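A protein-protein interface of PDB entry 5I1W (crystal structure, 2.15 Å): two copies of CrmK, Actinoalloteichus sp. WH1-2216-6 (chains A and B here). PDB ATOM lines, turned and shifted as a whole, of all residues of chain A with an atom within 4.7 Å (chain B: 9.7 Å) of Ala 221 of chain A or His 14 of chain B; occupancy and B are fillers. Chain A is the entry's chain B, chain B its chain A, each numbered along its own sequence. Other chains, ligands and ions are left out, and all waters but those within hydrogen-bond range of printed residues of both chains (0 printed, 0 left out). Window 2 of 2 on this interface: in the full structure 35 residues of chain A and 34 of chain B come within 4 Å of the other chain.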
ATOM      1  N   TYR A 112      -5.837   3.107  17.554  1.00  0.00           N
ATOM      2  CA  TYR A 112      -6.109   2.874  16.176  1.00  0.00           C
ATOM      3  C   TYR A 112      -4.831   2.781  15.353  1.00  0.00           C
ATOM      4  O   TYR A 112      -4.606   1.806  14.614  1.00  0.00           O
ATOM      5  CB  TYR A 112      -6.991   3.964  15.587  1.00  0.00           C
ATOM      6  CG  TYR A 112      -7.410   3.583  14.197  1.00  0.00           C
ATOM      7  CD1 TYR A 112      -8.278   2.518  13.988  1.00  0.00           C
ATOM      8  CD2 TYR A 112      -6.898   4.231  13.090  1.00  0.00           C
ATOM      9  CE1 TYR A 112      -8.656   2.137  12.709  1.00  0.00           C
ATOM     10  CE2 TYR A 112      -7.279   3.869  11.812  1.00  0.00           C
ATOM     11  CZ  TYR A 112      -8.156   2.827  11.634  1.00  0.00           C
ATOM     12  OH  TYR A 112      -8.519   2.471  10.375  1.00  0.00           O
ATOM     13  N   PRO A 219     -13.017  -0.539  13.841  1.00  0.00           N
ATOM     14  CA  PRO A 219     -14.071   0.233  13.243  1.00  0.00           C
ATOM     15  C   PRO A 219     -14.141  -0.021  11.751  1.00  0.00           C
ATOM     16  O   PRO A 219     -13.202  -0.579  11.186  1.00  0.00           O
ATOM     17  CB  PRO A 219     -13.638   1.681  13.506  1.00  0.00           C
ATOM     18  CG  PRO A 219     -12.164   1.634  13.640  1.00  0.00           C
ATOM     19  CD  PRO A 219     -11.866   0.291  14.248  1.00  0.00           C
ATOM     20  N   PRO A 220     -15.235   0.395  11.108  1.00  0.00           N
ATOM     21  CA  PRO A 220     -15.317   0.422   9.639  1.00  0.00           C
ATOM     22  C   PRO A 220     -14.289   1.418   9.090  1.00  0.00           C
ATOM     23  O   PRO A 220     -14.067   2.466   9.702  1.00  0.00           O
ATOM     24  CB  PRO A 220     -16.753   0.943   9.373  1.00  0.00           C
ATOM     25  CG  PRO A 220     -17.484   0.742  10.672  1.00  0.00           C
ATOM     26  CD  PRO A 220     -16.444   0.976  11.730  1.00  0.00           C
ATOM     27  N   ALA A 221     -13.653   1.109   7.970  1.00  0.00           N
ATOM     28  CA  ALA A 221     -12.509   1.920   7.530  1.00  0.00           C
ATOM     29  C   ALA A 221     -12.880   3.328   7.039  1.00  0.00           C
ATOM     30  O   ALA A 221     -12.102   4.266   7.192  1.00  0.00           O
ATOM     31  CB  ALA A 221     -11.755   1.189   6.438  1.00  0.00           C
ATOM     32  N   SER A 222     -14.058   3.472   6.448  1.00  0.00           N
ATOM     33  CA  SER A 222     -14.444   4.734   5.800  1.00  0.00           C
ATOM     34  C   SER A 222     -15.920   5.009   6.009  1.00  0.00           C
ATOM     35  O   SER A 222     -16.722   4.076   6.176  1.00  0.00           O
ATOM     36  CB  SER A 222     -14.155   4.673   4.283  1.00  0.00           C
ATOM     37  OG  SER A 222     -12.981   5.374   3.924  1.00  0.00           O
ATOM     38  N   PHE A 223     -16.267   6.290   6.013  1.00  0.00           N
ATOM     39  CA  PHE A 223     -17.613   6.719   6.296  1.00  0.00           C
ATOM     40  C   PHE A 223     -17.961   7.767   5.290  1.00  0.00           C
ATOM     41  O   PHE A 223     -17.091   8.588   4.967  1.00  0.00           O
ATOM     42  CB  PHE A 223     -17.713   7.381   7.682  1.00  0.00           C
ATOM     43  CG  PHE A 223     -17.769   6.414   8.820  1.00  0.00           C
ATOM     44  CD1 PHE A 223     -16.637   5.748   9.239  1.00  0.00           C
ATOM     45  CD2 PHE A 223     -18.952   6.191   9.492  1.00  0.00           C
ATOM     46  CE1 PHE A 223     -16.700   4.832  10.272  1.00  0.00           C
ATOM     47  CE2 PHE A 223     -19.017   5.293  10.532  1.00  0.00           C
ATOM     48  CZ  PHE A 223     -17.894   4.613  10.929  1.00  0.00           C
ATOM     49  N   LEU A 317     -14.523   9.912   4.303  1.00  0.00           N
ATOM     50  CA  LEU A 317     -13.279  10.022   5.064  1.00  0.00           C
ATOM     51  C   LEU A 317     -12.967   8.726   5.757  1.00  0.00           C
ATOM     52  O   LEU A 317     -13.867   7.964   6.004  1.00  0.00           O
ATOM     53  CB  LEU A 317     -13.403  11.132   6.102  1.00  0.00           C
ATOM     54  CG  LEU A 317     -13.437  12.570   5.550  1.00  0.00           C
ATOM     55  CD1 LEU A 317     -13.792  13.584   6.626  1.00  0.00           C
ATOM     56  CD2 LEU A 317     -12.109  12.941   4.911  1.00  0.00           C
ATOM     57  N   PRO A 318     -11.684   8.475   6.102  1.00  0.00           N
ATOM     58  CA  PRO A 318     -11.316   7.363   7.025  1.00  0.00           C
ATOM     59  C   PRO A 318     -11.977   7.519   8.405  1.00  0.00           C
ATOM     60  O   PRO A 318     -12.277   8.635   8.764  1.00  0.00           O
ATOM     61  CB  PRO A 318      -9.820   7.514   7.201  1.00  0.00           C
ATOM     62  CG  PRO A 318      -9.378   8.455   6.149  1.00  0.00           C
ATOM     63  CD  PRO A 318     -10.528   9.306   5.747  1.00  0.00           C
ATOM     64  N   TRP A 319     -12.207   6.432   9.156  1.00  0.00           N
ATOM     65  CA  TRP A 319     -12.909   6.544  10.456  1.00  0.00           C
ATOM     66  C   TRP A 319     -12.281   7.587  11.388  1.00  0.00           C
ATOM     67  O   TRP A 319     -12.957   8.504  11.871  1.00  0.00           O
ATOM     68  CB  TRP A 319     -13.005   5.205  11.214  1.00  0.00           C
ATOM     69  CG  TRP A 319     -13.411   5.447  12.639  1.00  0.00           C
ATOM     70  CD1 TRP A 319     -14.656   5.843  13.099  1.00  0.00           C
ATOM     71  CD2 TRP A 319     -12.551   5.459  13.780  1.00  0.00           C
ATOM     72  NE1 TRP A 319     -14.609   6.074  14.467  1.00  0.00           N
ATOM     73  CE2 TRP A 319     -13.341   5.825  14.908  1.00  0.00           C
ATOM     74  CE3 TRP A 319     -11.191   5.176  13.969  1.00  0.00           C
ATOM     75  CZ2 TRP A 319     -12.807   5.915  16.197  1.00  0.00           C
ATOM     76  CZ3 TRP A 319     -10.672   5.258  15.253  1.00  0.00           C
ATOM     77  CH2 TRP A 319     -11.473   5.622  16.346  1.00  0.00           C
ATOM     78  N   THR B   8       4.092  -2.349  10.270  1.00  0.00           N
ATOM     79  CA  THR B   8       4.209  -2.075   8.857  1.00  0.00           C
ATOM     80  C   THR B   8       2.791  -2.001   8.323  1.00  0.00           C
ATOM     81  O   THR B   8       1.989  -2.859   8.632  1.00  0.00           O
ATOM     82  CB  THR B   8       5.060  -3.152   8.165  1.00  0.00           C
ATOM     83  OG1 THR B   8       6.414  -2.995   8.596  1.00  0.00           O
ATOM     84  CG2 THR B   8       5.033  -3.040   6.657  1.00  0.00           C
ATOM     85  N   VAL B   9       2.463  -0.955   7.575  1.00  0.00           N
ATOM     86  CA  VAL B   9       1.093  -0.736   7.133  1.00  0.00           C
ATOM     87  C   VAL B   9       1.122  -0.648   5.619  1.00  0.00           C
ATOM     88  O   VAL B   9       1.661   0.290   5.061  1.00  0.00           O
ATOM     89  CB  VAL B   9       0.499   0.546   7.725  1.00  0.00           C
ATOM     90  CG1 VAL B   9      -0.925   0.783   7.217  1.00  0.00           C
ATOM     91  CG2 VAL B   9       0.502   0.487   9.221  1.00  0.00           C
ATOM     92  N   LYS B  10       0.585  -1.673   4.962  1.00  0.00           N
ATOM     93  CA  LYS B  10       0.554  -1.753   3.517  1.00  0.00           C
ATOM     94  C   LYS B  10      -0.817  -1.341   3.028  1.00  0.00           C
ATOM     95  O   LYS B  10      -1.734  -1.217   3.822  1.00  0.00           O
ATOM     96  CB  LYS B  10       0.881  -3.164   3.060  1.00  0.00           C
ATOM     97  CG  LYS B  10       2.242  -3.576   3.532  1.00  0.00           C
ATOM     98  CD  LYS B  10       2.946  -4.465   2.531  1.00  0.00           C
ATOM     99  CE  LYS B  10       4.285  -4.925   3.068  1.00  0.00           C
ATOM    100  NZ  LYS B  10       4.086  -6.191   3.835  1.00  0.00           N
ATOM    101  N   PRO B  11      -0.951  -1.119   1.725  1.00  0.00           N
ATOM    102  CA  PRO B  11      -2.215  -0.604   1.158  1.00  0.00           C
ATOM    103  C   PRO B  11      -3.456  -1.420   1.396  1.00  0.00           C
ATOM    104  O   PRO B  11      -4.563  -0.895   1.239  1.00  0.00           O
ATOM    105  CB  PRO B  11      -1.947  -0.558  -0.341  1.00  0.00           C
ATOM    106  CG  PRO B  11      -0.465  -0.417  -0.442  1.00  0.00           C
ATOM    107  CD  PRO B  11       0.120  -1.191   0.720  1.00  0.00           C
ATOM    108  N   ASP B  12      -3.281  -2.694   1.729  1.00  0.00           N
ATOM    109  CA  ASP B  12      -4.402  -3.583   2.090  1.00  0.00           C
ATOM    110  C   ASP B  12      -4.857  -3.478   3.554  1.00  0.00           C
ATOM    111  O   ASP B  12      -5.860  -4.061   3.921  1.00  0.00           O
ATOM    112  CB  ASP B  12      -4.025  -5.050   1.797  1.00  0.00           C
ATOM    113  CG  ASP B  12      -2.818  -5.536   2.619  1.00  0.00           C
ATOM    114  OD1 ASP B  12      -1.866  -4.754   2.823  1.00  0.00           O
ATOM    115  OD2 ASP B  12      -2.813  -6.704   3.066  1.00  0.00           O
ATOM    116  N   ASP B  13      -4.084  -2.793   4.397  1.00  0.00           N
ATOM    117  CA  ASP B  13      -4.410  -2.619   5.808  1.00  0.00           C
ATOM    118  C   ASP B  13      -5.321  -1.432   5.922  1.00  0.00           C
ATOM    119  O   ASP B  13      -5.153  -0.423   5.239  1.00  0.00           O
ATOM    120  CB  ASP B  13      -3.126  -2.436   6.622  1.00  0.00           C
ATOM    121  CG  ASP B  13      -3.363  -2.261   8.107  1.00  0.00           C
ATOM    122  OD1 ASP B  13      -4.088  -1.334   8.563  1.00  0.00           O
ATOM    123  OD2 ASP B  13      -2.747  -3.021   8.873  1.00  0.00           O
ATOM    124  N   HIS B  14      -6.295  -1.534   6.817  1.00  0.00           N
ATOM    125  CA  HIS B  14      -7.301  -0.503   6.919  1.00  0.00           C
ATOM    126  C   HIS B  14      -6.720   0.825   7.319  1.00  0.00           C
ATOM    127  O   HIS B  14      -7.233   1.869   6.881  1.00  0.00           O
ATOM    128  CB  HIS B  14      -8.480  -0.943   7.818  1.00  0.00           C
ATOM    129  CG  HIS B  14      -9.427  -1.864   7.105  1.00  0.00           C
ATOM    130  ND1 HIS B  14      -9.857  -3.064   7.636  1.00  0.00           N
ATOM    131  CD2 HIS B  14      -9.957  -1.794   5.859  1.00  0.00           C
ATOM    132  CE1 HIS B  14     -10.637  -3.675   6.761  1.00  0.00           C
ATOM    133  NE2 HIS B  14     -10.719  -2.923   5.677  1.00  0.00           N
ATOM    134  N   ARG B  15      -5.612   0.791   8.076  1.00  0.00           N
ATOM    135  CA  ARG B  15      -4.944   2.037   8.522  1.00  0.00           C
ATOM    136  C   ARG B  15      -4.255   2.864   7.442  1.00  0.00           C
ATOM    137  O   ARG B  15      -3.963   4.073   7.665  1.00  0.00           O
ATOM    138  CB  ARG B  15      -3.880   1.698   9.548  1.00  0.00           C
ATOM    139  CG  ARG B  15      -4.392   1.280  10.888  1.00  0.00           C
ATOM    140  CD  ARG B  15      -3.256   0.755  11.748  1.00  0.00           C
ATOM    141  NE  ARG B  15      -2.839  -0.545  11.311  1.00  0.00           N
ATOM    142  CZ  ARG B  15      -2.047  -1.350  12.006  1.00  0.00           C
ATOM    143  NH1 ARG B  15      -1.588  -1.016  13.189  1.00  0.00           N
ATOM    144  NH2 ARG B  15      -1.719  -2.513  11.506  1.00  0.00           N
ATOM    145  N   TYR B  16      -3.936   2.223   6.304  1.00  0.00           N
ATOM    146  CA  TYR B  16      -3.116   2.878   5.287  1.00  0.00           C
ATOM    147  C   TYR B  16      -3.750   4.190   4.827  1.00  0.00           C
ATOM    148  O   TYR B  16      -3.068   5.207   4.783  1.00  0.00           O
ATOM    149  CB  TYR B  16      -2.913   1.938   4.114  1.00  0.00           C
ATOM    150  CG  TYR B  16      -2.036   2.428   2.967  1.00  0.00           C
ATOM    151  CD1 TYR B  16      -2.593   3.168   1.879  1.00  0.00           C
ATOM    152  CD2 TYR B  16      -0.682   2.078   2.904  1.00  0.00           C
ATOM    153  CE1 TYR B  16      -1.808   3.583   0.815  1.00  0.00           C
ATOM    154  CE2 TYR B  16       0.112   2.505   1.822  1.00  0.00           C
ATOM    155  CZ  TYR B  16      -0.466   3.261   0.794  1.00  0.00           C
ATOM    156  OH  TYR B  16       0.303   3.657  -0.266  1.00  0.00           O
ATOM    157  N   ASP B  17      -5.040   4.196   4.509  1.00  0.00           N
ATOM    158  CA  ASP B  17      -5.679   5.421   4.006  1.00  0.00           C
ATOM    159  C   ASP B  17      -5.683   6.541   5.040  1.00  0.00           C
ATOM    160  O   ASP B  17      -5.575   7.725   4.711  1.00  0.00           O
ATOM    161  CB  ASP B  17      -7.103   5.137   3.480  1.00  0.00           C
ATOM    162  CG  ASP B  17      -7.107   4.186   2.229  1.00  0.00           C
ATOM    163  OD1 ASP B  17      -6.043   3.988   1.579  1.00  0.00           O
ATOM    164  OD2 ASP B  17      -8.173   3.621   1.892  1.00  0.00           O
ATOM    165  N   LEU B  18      -5.719   6.201   6.304  1.00  0.00           N
ATOM    166  CA  LEU B  18      -5.619   7.277   7.313  1.00  0.00           C
ATOM    167  C   LEU B  18      -4.191   7.862   7.399  1.00  0.00           C
ATOM    168  O   LEU B  18      -3.988   9.074   7.407  1.00  0.00           O
ATOM    169  CB  LEU B  18      -6.032   6.750   8.667  1.00  0.00           C
ATOM    170  CG  LEU B  18      -5.691   7.792   9.749  1.00  0.00           C
ATOM    171  CD1 LEU B  18      -6.626   8.995   9.676  1.00  0.00           C
ATOM    172  CD2 LEU B  18      -5.668   7.138  11.128  1.00  0.00           C
ATOM    173  N   LEU B  19      -3.198   6.979   7.477  1.00  0.00           N
ATOM    174  CA  LEU B  19      -1.794   7.408   7.467  1.00  0.00           C
ATOM    175  C   LEU B  19      -1.349   8.186   6.221  1.00  0.00           C
ATOM    176  O   LEU B  19      -0.461   9.048   6.282  1.00  0.00           O
ATOM    177  CB  LEU B  19      -0.907   6.202   7.647  1.00  0.00           C
ATOM    178  CG  LEU B  19      -1.041   5.600   9.022  1.00  0.00           C
ATOM    179  CD1 LEU B  19      -0.157   4.387   9.149  1.00  0.00           C
ATOM    180  CD2 LEU B  19      -0.673   6.623  10.074  1.00  0.00           C
ATOM    181  N   ALA B  20      -1.989   7.909   5.097  1.00  0.00           N
ATOM    182  CA  ALA B  20      -1.762   8.637   3.901  1.00  0.00           C
ATOM    183  C   ALA B  20      -2.198  10.117   3.993  1.00  0.00           C
ATOM    184  O   ALA B  20      -1.808  10.941   3.165  1.00  0.00           O
ATOM    185  CB  ALA B  20      -2.499   7.950   2.771  1.00  0.00           C
ATOM    186  N   ARG B  21      -2.994  10.462   4.988  1.00  0.00           N
ATOM    187  CA  ARG B  21      -3.574  11.789   5.082  1.00  0.00           C
ATOM    188  C   ARG B  21      -3.002  12.506   6.295  1.00  0.00           C
ATOM    189  O   ARG B  21      -2.888  11.902   7.363  1.00  0.00           O
ATOM    190  CB  ARG B  21      -5.092  11.639   5.228  1.00  0.00           C
ATOM    191  CG  ARG B  21      -5.741  11.355   3.892  1.00  0.00           C
ATOM    192  CD  ARG B  21      -7.106  10.673   3.974  1.00  0.00           C
ATOM    193  NE  ARG B  21      -7.596  10.583   2.608  1.00  0.00           N
ATOM    194  CZ  ARG B  21      -7.235   9.652   1.727  1.00  0.00           C
ATOM    195  NH1 ARG B  21      -6.438   8.635   2.061  1.00  0.00           N
ATOM    196  NH2 ARG B  21      -7.692   9.730   0.489  1.00  0.00           N
ATOM    197  N   TYR B  25      -4.831  18.138   3.022  1.00  0.00           N
ATOM    198  CA  TYR B  25      -5.490  17.160   2.160  1.00  0.00           C
ATOM    199  C   TYR B  25      -5.197  17.292   0.676  1.00  0.00           C
ATOM    200  O   TYR B  25      -5.582  16.418  -0.124  1.00  0.00           O
ATOM    201  CB  TYR B  25      -7.020  17.086   2.421  1.00  0.00           C
ATOM    202  CG  TYR B  25      -7.422  16.016   3.433  1.00  0.00           C
ATOM    203  CD1 TYR B  25      -6.729  15.883   4.654  1.00  0.00           C
ATOM    204  CD2 TYR B  25      -8.485  15.143   3.186  1.00  0.00           C
ATOM    205  CE1 TYR B  25      -7.077  14.923   5.570  1.00  0.00           C
ATOM    206  CE2 TYR B  25      -8.847  14.180   4.118  1.00  0.00           C
ATOM    207  CZ  TYR B  25      -8.145  14.077   5.304  1.00  0.00           C
ATOM    208  OH  TYR B  25      -8.496  13.137   6.239  1.00  0.00           O
ATOM    209  N   PHE B  34       3.889   2.280   5.245  1.00  0.00           N
ATOM    210  CA  PHE B  34       4.230   3.109   6.361  1.00  0.00           C
ATOM    211  C   PHE B  34       4.903   2.200   7.396  1.00  0.00           C
ATOM    212  O   PHE B  34       4.501   1.068   7.594  1.00  0.00           O
ATOM    213  CB  PHE B  34       3.012   3.746   6.967  1.00  0.00           C
ATOM    214  CG  PHE B  34       2.281   4.639   6.047  1.00  0.00           C
ATOM    215  CD1 PHE B  34       1.274   4.157   5.274  1.00  0.00           C
ATOM    216  CD2 PHE B  34       2.588   5.968   5.975  1.00  0.00           C
ATOM    217  CE1 PHE B  34       0.585   4.988   4.428  1.00  0.00           C
ATOM    218  CE2 PHE B  34       1.918   6.809   5.139  1.00  0.00           C
ATOM    219  CZ  PHE B  34       0.943   6.311   4.332  1.00  0.00           C
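The guanidinium group of Arg 15 of chain B is in salt-bridge range of the side-chain carboxylate of Asp 13 of chain B, 2.9 Å away. The backbone NH of Phe 223 of chain A lies within hydrogen-bond range of the backbone carbonyl oxygen of Leu 317 of chain A, at 2.9 Å. The backbone carbonyl oxygen (O) of Asp 17 of chain B sits at hydrogen-bond distance from the guanidinium group (NH1) of Arg 21 of chain B, at 2.9 Å. O of Ala 221 of chain A is in hydrogen-bond range of N of Trp 319 of chain A (2.9 Å). The backbone carbonyl oxygen of Leu 317 of chain A lies close to the side-chain hydroxyl of Ser 222 of chain A.
Among the printed residues, pairs that only touch across the chains: Tyr 112 of chain A with Arg 15 of chain B (3.3 Å), Ala 221 of chain A with His 14 of chain B (3.5 Å), Leu 317 of chain A with Tyr 25 of chain B (3.6 Å), Tyr 112 of chain A with Leu 18 of chain B (3.7 Å), Tyr 112 of chain A with His 14 of chain B (3.8 Å) and Pro 318 of chain A with Arg 21 of chain B (3.8 Å).
Printed residues of chain B within 4 Å of Tyr 112 of chain A: His 14 (3.8 Å), Arg 15 (3.3 Å) and Leu 18 (3.7 Å). No residue of chain B comes within 4 Å of Pro 220 of chain A. Ala 221 of chain A touches just one residue of chain B: His 14 (3.5 Å). No residue of chain B comes within 4 Å of Ser 222 of chain A. Of the printed residues of chain B, Leu 317 of chain A touches Tyr 25. Of chain B, only Arg 21 comes within 4 Å of Pro 318 of chain A. Printed residues of chain A within 4 Å of Arg 15 of chain B: Tyr 112 (3.3 Å). Of the printed residues of chain A, Leu 18 of chain B touches Tyr 112. Leu 19 of chain B touches none of the printed residues of chain A. Of the printed residues of chain A, Arg 21 of chain B touches Pro 318. The nearest printed residue of chain A that does not touch His 14 of chain B is Pro 219 of chain A (5.5 Å).
Along chain A the printed residues that touch a printed residue of chain B span positions 112 to 318. Of the 16 printed residues of chain B, 5 touch a printed residue of chain A. Hydrophobic or aromatic side chains of chain B within 4 Å of the printed part of chain A: His 14, Leu 18 and Tyr 25. Among the printed residues, 6 pairs touch across the chains. Among the printed residues, no Asp or Glu carboxylate lies within 4 Å of a Lys or Arg side-chain nitrogen of the other chain.
No position is printed for both chains. Of the 6 pairs that touch across the chains among the printed residues, none has its exchanged pair printed and touching as well.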
